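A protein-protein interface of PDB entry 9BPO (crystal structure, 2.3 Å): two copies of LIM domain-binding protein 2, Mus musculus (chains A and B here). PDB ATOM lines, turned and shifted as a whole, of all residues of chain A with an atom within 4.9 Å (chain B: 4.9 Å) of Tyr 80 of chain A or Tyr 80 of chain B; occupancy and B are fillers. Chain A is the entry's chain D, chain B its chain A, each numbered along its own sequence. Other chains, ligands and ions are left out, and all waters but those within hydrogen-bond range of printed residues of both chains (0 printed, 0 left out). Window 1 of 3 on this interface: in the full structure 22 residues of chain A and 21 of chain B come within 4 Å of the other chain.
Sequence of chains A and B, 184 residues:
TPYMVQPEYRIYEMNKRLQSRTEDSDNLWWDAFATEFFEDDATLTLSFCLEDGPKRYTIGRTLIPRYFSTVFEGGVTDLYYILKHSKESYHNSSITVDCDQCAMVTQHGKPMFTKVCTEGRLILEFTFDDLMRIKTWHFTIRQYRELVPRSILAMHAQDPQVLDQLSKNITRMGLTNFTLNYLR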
ATOM      1  N   ASN A  15       8.240   9.311 -36.690  1.00  0.00           N
ATOM      2  CA  ASN A  15       9.294  10.235 -36.295  1.00  0.00           C
ATOM      3  C   ASN A  15       9.936  10.860 -37.523  1.00  0.00           C
ATOM      4  O   ASN A  15      10.048  12.085 -37.613  1.00  0.00           O
ATOM      5  CB  ASN A  15      10.342   9.523 -35.431  1.00  0.00           C
ATOM      6  CG  ASN A  15       9.877   9.326 -33.973  1.00  0.00           C
ATOM      7  OD1 ASN A  15       8.796   9.778 -33.582  1.00  0.00           O
ATOM      8  ND2 ASN A  15      10.688   8.635 -33.181  1.00  0.00           N
ATOM      9  N   ASP A  78      11.148  20.275 -32.854  1.00  0.00           N
ATOM     10  CA  ASP A  78      11.240  18.831 -33.041  1.00  0.00           C
ATOM     11  C   ASP A  78      10.270  18.133 -32.114  1.00  0.00           C
ATOM     12  O   ASP A  78      10.027  18.584 -30.991  1.00  0.00           O
ATOM     13  CB  ASP A  78      12.625  18.296 -32.755  1.00  0.00           C
ATOM     14  CG  ASP A  78      13.637  18.744 -33.773  1.00  0.00           C
ATOM     15  OD1 ASP A  78      14.839  18.774 -33.420  1.00  0.00           O
ATOM     16  OD2 ASP A  78      13.255  19.050 -34.929  1.00  0.00           O
ATOM     17  N   LEU A  79       9.737  17.012 -32.592  1.00  0.00           N
ATOM     18  CA  LEU A  79       8.925  16.124 -31.773  1.00  0.00           C
ATOM     19  C   LEU A  79       9.151  14.700 -32.248  1.00  0.00           C
ATOM     20  O   LEU A  79       8.956  14.405 -33.431  1.00  0.00           O
ATOM     21  CB  LEU A  79       7.457  16.485 -31.861  1.00  0.00           C
ATOM     22  CG  LEU A  79       6.585  15.320 -31.442  1.00  0.00           C
ATOM     23  CD1 LEU A  79       6.541  15.275 -29.967  1.00  0.00           C
ATOM     24  CD2 LEU A  79       5.202  15.542 -31.992  1.00  0.00           C
ATOM     25  N   TYR A  80       9.568  13.823 -31.340  1.00  0.00           N
ATOM     26  CA  TYR A  80       9.745  12.428 -31.701  1.00  0.00           C
ATOM     27  C   TYR A  80       9.421  11.561 -30.490  1.00  0.00           C
ATOM     28  O   TYR A  80       9.334  12.048 -29.350  1.00  0.00           O
ATOM     29  CB  TYR A  80      11.158  12.166 -32.248  1.00  0.00           C
ATOM     30  CG  TYR A  80      12.283  12.567 -31.327  1.00  0.00           C
ATOM     31  CD1 TYR A  80      12.711  11.704 -30.317  1.00  0.00           C
ATOM     32  CD2 TYR A  80      12.945  13.793 -31.475  1.00  0.00           C
ATOM     33  CE1 TYR A  80      13.748  12.038 -29.466  1.00  0.00           C
ATOM     34  CE2 TYR A  80      13.996  14.150 -30.602  1.00  0.00           C
ATOM     35  CZ  TYR A  80      14.388  13.255 -29.604  1.00  0.00           C
ATOM     36  OH  TYR A  80      15.409  13.541 -28.726  1.00  0.00           O
ATOM     37  N   TYR A  81       9.211  10.266 -30.753  1.00  0.00           N
ATOM     38  CA  TYR A  81       8.868   9.307 -29.715  1.00  0.00           C
ATOM     39  C   TYR A  81       9.970   8.266 -29.595  1.00  0.00           C
ATOM     40  O   TYR A  81      10.475   7.757 -30.600  1.00  0.00           O
ATOM     41  CB  TYR A  81       7.521   8.640 -29.991  1.00  0.00           C
ATOM     42  CG  TYR A  81       6.355   9.604 -29.951  1.00  0.00           C
ATOM     43  CD1 TYR A  81       5.997  10.322 -31.078  1.00  0.00           C
ATOM     44  CD2 TYR A  81       5.623   9.819 -28.782  1.00  0.00           C
ATOM     45  CE1 TYR A  81       4.939  11.214 -31.058  1.00  0.00           C
ATOM     46  CE2 TYR A  81       4.550  10.718 -28.751  1.00  0.00           C
ATOM     47  CZ  TYR A  81       4.230  11.416 -29.898  1.00  0.00           C
ATOM     48  OH  TYR A  81       3.192  12.313 -29.927  1.00  0.00           O
ATOM     49  N   ILE A  82      10.349   7.974 -28.363  1.00  0.00           N
ATOM     50  CA  ILE A  82      11.328   6.948 -28.041  1.00  0.00           C
ATOM     51  C   ILE A  82      10.584   5.832 -27.329  1.00  0.00           C
ATOM     52  O   ILE A  82      10.031   6.061 -26.249  1.00  0.00           O
ATOM     53  CB  ILE A  82      12.447   7.498 -27.143  1.00  0.00           C
ATOM     54  CG1 ILE A  82      13.084   8.724 -27.790  1.00  0.00           C
ATOM     55  CG2 ILE A  82      13.408   6.378 -26.718  1.00  0.00           C
ATOM     56  CD1 ILE A  82      13.883   8.365 -29.041  1.00  0.00           C
ATOM     57  N   ALA A 103       8.802   7.754 -24.283  1.00  0.00           N
ATOM     58  CA  ALA A 103       9.235   9.121 -24.029  1.00  0.00           C
ATOM     59  C   ALA A 103       8.792   9.964 -25.208  1.00  0.00           C
ATOM     60  O   ALA A 103       9.162   9.688 -26.349  1.00  0.00           O
ATOM     61  CB  ALA A 103      10.750   9.204 -23.831  1.00  0.00           C
ATOM     62  N   MET A 104       7.973  10.958 -24.941  1.00  0.00           N
ATOM     63  CA  MET A 104       7.618  11.944 -25.942  1.00  0.00           C
ATOM     64  C   MET A 104       8.534  13.147 -25.721  1.00  0.00           C
ATOM     65  O   MET A 104       8.531  13.750 -24.639  1.00  0.00           O
ATOM     66  CB  MET A 104       6.136  12.294 -25.824  1.00  0.00           C
ATOM     67  CG  MET A 104       5.653  13.372 -26.760  1.00  0.00           C
ATOM     68  SD  MET A 104       3.960  13.822 -26.305  1.00  0.00           S
ATOM     69  CE  MET A 104       3.817  15.363 -27.209  1.00  0.00           C
ATOM     70  N   VAL A 105       9.361  13.456 -26.715  1.00  0.00           N
ATOM     71  CA  VAL A 105      10.390  14.475 -26.590  1.00  0.00           C
ATOM     72  C   VAL A 105      10.059  15.622 -27.536  1.00  0.00           C
ATOM     73  O   VAL A 105       9.773  15.392 -28.722  1.00  0.00           O
ATOM     74  CB  VAL A 105      11.790  13.901 -26.876  1.00  0.00           C
ATOM     75  CG1 VAL A 105      12.829  14.930 -26.514  1.00  0.00           C
ATOM     76  CG2 VAL A 105      12.020  12.631 -26.072  1.00  0.00           C
ATOM     77  N   LYS A 115      14.284  21.272 -23.589  1.00  0.00           N
ATOM     78  CA  LYS A 115      13.909  19.946 -24.087  1.00  0.00           C
ATOM     79  C   LYS A 115      12.970  19.310 -23.081  1.00  0.00           C
ATOM     80  O   LYS A 115      13.360  19.081 -21.929  1.00  0.00           O
ATOM     81  CB  LYS A 115      15.112  19.051 -24.295  1.00  0.00           C
ATOM     82  CG  LYS A 115      14.814  17.876 -25.155  1.00  0.00           C
ATOM     83  CD  LYS A 115      16.063  17.078 -25.321  1.00  0.00           C
ATOM     84  CE  LYS A 115      16.771  17.508 -26.576  1.00  0.00           C
ATOM     85  NZ  LYS A 115      18.019  16.700 -26.766  1.00  0.00           N
ATOM     86  N   ASN B  15      19.713   1.385 -32.454  1.00  0.00           N
ATOM     87  CA  ASN B  15      19.100   2.008 -31.282  1.00  0.00           C
ATOM     88  C   ASN B  15      18.379   0.972 -30.417  1.00  0.00           C
ATOM     89  O   ASN B  15      18.524   0.961 -29.189  1.00  0.00           O
ATOM     90  CB  ASN B  15      18.129   3.106 -31.723  1.00  0.00           C
ATOM     91  CG  ASN B  15      18.825   4.388 -32.135  1.00  0.00           C
ATOM     92  OD1 ASN B  15      19.963   4.654 -31.746  1.00  0.00           O
ATOM     93  ND2 ASN B  15      18.141   5.195 -32.937  1.00  0.00           N
ATOM     94  N   ASP B  78      21.121   5.540 -21.085  1.00  0.00           N
ATOM     95  CA  ASP B  78      20.533   5.476 -22.415  1.00  0.00           C
ATOM     96  C   ASP B  78      21.472   6.155 -23.399  1.00  0.00           C
ATOM     97  O   ASP B  78      22.100   7.165 -23.068  1.00  0.00           O
ATOM     98  CB  ASP B  78      19.170   6.185 -22.474  1.00  0.00           C
ATOM     99  CG  ASP B  78      18.094   5.471 -21.682  1.00  0.00           C
ATOM    100  OD1 ASP B  78      17.636   4.383 -22.111  1.00  0.00           O
ATOM    101  OD2 ASP B  78      17.749   5.986 -20.584  1.00  0.00           O
ATOM    102  N   LEU B  79      21.560   5.597 -24.600  1.00  0.00           N
ATOM    103  CA  LEU B  79      22.233   6.243 -25.714  1.00  0.00           C
ATOM    104  C   LEU B  79      21.454   5.917 -26.974  1.00  0.00           C
ATOM    105  O   LEU B  79      21.194   4.748 -27.236  1.00  0.00           O
ATOM    106  CB  LEU B  79      23.688   5.775 -25.861  1.00  0.00           C
ATOM    107  CG  LEU B  79      24.276   5.932 -27.271  1.00  0.00           C
ATOM    108  CD1 LEU B  79      24.474   7.379 -27.664  1.00  0.00           C
ATOM    109  CD2 LEU B  79      25.593   5.216 -27.367  1.00  0.00           C
ATOM    110  N   TYR B  80      21.100   6.927 -27.759  1.00  0.00           N
ATOM    111  CA  TYR B  80      20.460   6.668 -29.040  1.00  0.00           C
ATOM    112  C   TYR B  80      20.840   7.763 -30.027  1.00  0.00           C
ATOM    113  O   TYR B  80      21.431   8.784 -29.662  1.00  0.00           O
ATOM    114  CB  TYR B  80      18.945   6.564 -28.901  1.00  0.00           C
ATOM    115  CG  TYR B  80      18.305   7.741 -28.200  1.00  0.00           C
ATOM    116  CD1 TYR B  80      17.983   8.892 -28.913  1.00  0.00           C
ATOM    117  CD2 TYR B  80      18.006   7.703 -26.845  1.00  0.00           C
ATOM    118  CE1 TYR B  80      17.380   9.970 -28.311  1.00  0.00           C
ATOM    119  CE2 TYR B  80      17.379   8.786 -26.223  1.00  0.00           C
ATOM    120  CZ  TYR B  80      17.072   9.918 -26.970  1.00  0.00           C
ATOM    121  OH  TYR B  80      16.473  11.028 -26.412  1.00  0.00           O
ATOM    122  N   TYR B  81      20.465   7.535 -31.290  1.00  0.00           N
ATOM    123  CA  TYR B  81      20.827   8.393 -32.411  1.00  0.00           C
ATOM    124  C   TYR B  81      19.574   8.866 -33.123  1.00  0.00           C
ATOM    125  O   TYR B  81      18.747   8.050 -33.531  1.00  0.00           O
ATOM    126  CB  TYR B  81      21.745   7.648 -33.386  1.00  0.00           C
ATOM    127  CG  TYR B  81      23.113   7.444 -32.788  1.00  0.00           C
ATOM    128  CD1 TYR B  81      24.094   8.410 -32.907  1.00  0.00           C
ATOM    129  CD2 TYR B  81      23.418   6.290 -32.086  1.00  0.00           C
ATOM    130  CE1 TYR B  81      25.341   8.235 -32.327  1.00  0.00           C
ATOM    131  CE2 TYR B  81      24.661   6.106 -31.515  1.00  0.00           C
ATOM    132  CZ  TYR B  81      25.610   7.083 -31.629  1.00  0.00           C
ATOM    133  OH  TYR B  81      26.840   6.880 -31.063  1.00  0.00           O
ATOM    134  N   ILE B  82      19.437  10.181 -33.275  1.00  0.00           N
ATOM    135  CA  ILE B  82      18.384  10.792 -34.084  1.00  0.00           C
ATOM    136  C   ILE B  82      19.042  11.329 -35.344  1.00  0.00           C
ATOM    137  O   ILE B  82      19.916  12.202 -35.266  1.00  0.00           O
ATOM    138  CB  ILE B  82      17.666  11.923 -33.328  1.00  0.00           C
ATOM    139  CG1 ILE B  82      17.426  11.536 -31.863  1.00  0.00           C
ATOM    140  CG2 ILE B  82      16.372  12.320 -34.021  1.00  0.00           C
ATOM    141  CD1 ILE B  82      16.233  10.666 -31.680  1.00  0.00           C
ATOM    142  N   ALA B 103      21.942  13.644 -34.077  1.00  0.00           N
ATOM    143  CA  ALA B 103      22.036  13.936 -32.656  1.00  0.00           C
ATOM    144  C   ALA B 103      22.329  12.646 -31.907  1.00  0.00           C
ATOM    145  O   ALA B 103      21.566  11.675 -31.990  1.00  0.00           O
ATOM    146  CB  ALA B 103      20.758  14.593 -32.139  1.00  0.00           C
ATOM    147  N   MET B 104      23.422  12.635 -31.171  1.00  0.00           N
ATOM    148  CA  MET B 104      23.715  11.519 -30.295  1.00  0.00           C
ATOM    149  C   MET B 104      23.359  11.920 -28.860  1.00  0.00           C
ATOM    150  O   MET B 104      23.873  12.922 -28.330  1.00  0.00           O
ATOM    151  CB  MET B 104      25.171  11.111 -30.444  1.00  0.00           C
ATOM    152  CG  MET B 104      25.688  10.313 -29.290  1.00  0.00           C
ATOM    153  SD  MET B 104      27.455  10.157 -29.504  1.00  0.00           S
ATOM    154  CE  MET B 104      27.882   9.678 -27.822  1.00  0.00           C
ATOM    155  N   VAL B 105      22.456  11.151 -28.254  1.00  0.00           N
ATOM    156  CA  VAL B 105      21.802  11.494 -27.004  1.00  0.00           C
ATOM    157  C   VAL B 105      22.224  10.470 -25.967  1.00  0.00           C
ATOM    158  O   VAL B 105      22.146   9.264 -26.221  1.00  0.00           O
ATOM    159  CB  VAL B 105      20.272  11.507 -27.175  1.00  0.00           C
ATOM    160  CG1 VAL B 105      19.582  11.940 -25.903  1.00  0.00           C
ATOM    161  CG2 VAL B 105      19.874  12.408 -28.341  1.00  0.00           C
ATOM    162  N   LYS B 115      20.825  15.150 -19.486  1.00  0.00           N
ATOM    163  CA  LYS B 115      20.690  14.661 -20.849  1.00  0.00           C
ATOM    164  C   LYS B 115      21.708  15.377 -21.735  1.00  0.00           C
ATOM    165  O   LYS B 115      21.636  16.601 -21.907  1.00  0.00           O
ATOM    166  CB  LYS B 115      19.272  14.869 -21.382  1.00  0.00           C
ATOM    167  CG  LYS B 115      19.083  14.223 -22.763  1.00  0.00           C
ATOM    168  CD  LYS B 115      17.648  14.229 -23.202  1.00  0.00           C
ATOM    169  CE  LYS B 115      16.837  13.167 -22.469  1.00  0.00           C
ATOM    170  NZ  LYS B 115      15.381  13.266 -22.841  1.00  0.00           N
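The backbone NH (N) of Ala 103 of chain B is in hydrogen-bond range of the backbone carbonyl oxygen (O) of Ile 82 of chain B, 2.8 Å away. O of Ile 82 of chain A lies within hydrogen-bond range of N of Ala 103 of chain A (2.9 Å). O of Tyr 80 of chain A lies within hydrogen-bond range of N of Val 105 of chain A (3.0 Å). O of Tyr 80 of chain B is in hydrogen-bond range of N of Val 105 of chain B (2.9 Å).
Tyr 80 of chain B touches Tyr 80 of chain A (OH to OH, 3.6 Å). Tyr 80 of chain A touches Ile 82 of chain B. CD1 of Ile 82 of chain A touches CE1 of Tyr 80 of chain B (3.9 Å). Lys 115 of chain B touches Lys 115 of chain A.
Of chain B, only Tyr 80 and Ile 82 come within 4 Å of Tyr 80 of chain A. Of the printed residues of chain B, Ile 82 of chain A touches Tyr 80 (3.9 Å). Met 104 of chain A touches none of the printed residues of chain B. Printed residues of chain B within 4 Å of Lys 115 of chain A: Lys 115. Tyr 80 of chain B touches just these residues of chain A: Tyr 80 (3.6 Å) and Ile 82 (3.9 Å). Of the printed residues of chain A, Ile 82 of chain B touches Tyr 80 (3.6 Å). Ala 103 of chain B touches none of the printed residues of chain A. Of the printed residues of chain A, Lys 115 of chain B touches Lys 115 (3.9 Å). The nearest residue of chain B that does not touch Tyr 80 of chain A is Val 105 of chain B (4.6 Å). The nearest residue of chain A that does not touch Tyr 80 of chain B is Val 105 of chain A (4.7 Å). The nearest printed residue of chain A that does not touch Ile 82 of chain B is Ile 82 of chain A (4.2 Å).
Hydrophobic or aromatic side chains of chain B within 4 Å of the printed part of chain A: Tyr 80 and Ile 82. Printed residues of chain A that touch a printed residue of chain B: Tyr 80, Ile 82 and Lys 115. Hydrophobic or aromatic side chains of chain A within 4 Å of the printed part of chain B: Tyr 80 and Ile 82. Among the printed residues, 4 pairs touch across the chains. Among the printed residues, no Asp or Glu carboxylate lies within 4 Å of a Lys or Arg side-chain nitrogen of the other chain.
Tyr 80 of chain B touches its own counterpart, Tyr 80 of chain A. Tyr 80 of chain A touches Ile 82 of chain B, and with the chains exchanged Ile 82 of chain A touches Tyr 80 of chain B. Lys 115 of chain B touches its own counterpart, Lys 115 of chain A. Of the 4 pairs that touch across the chains among the printed residues, 4 have their exchanged pair printed and touching as well.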
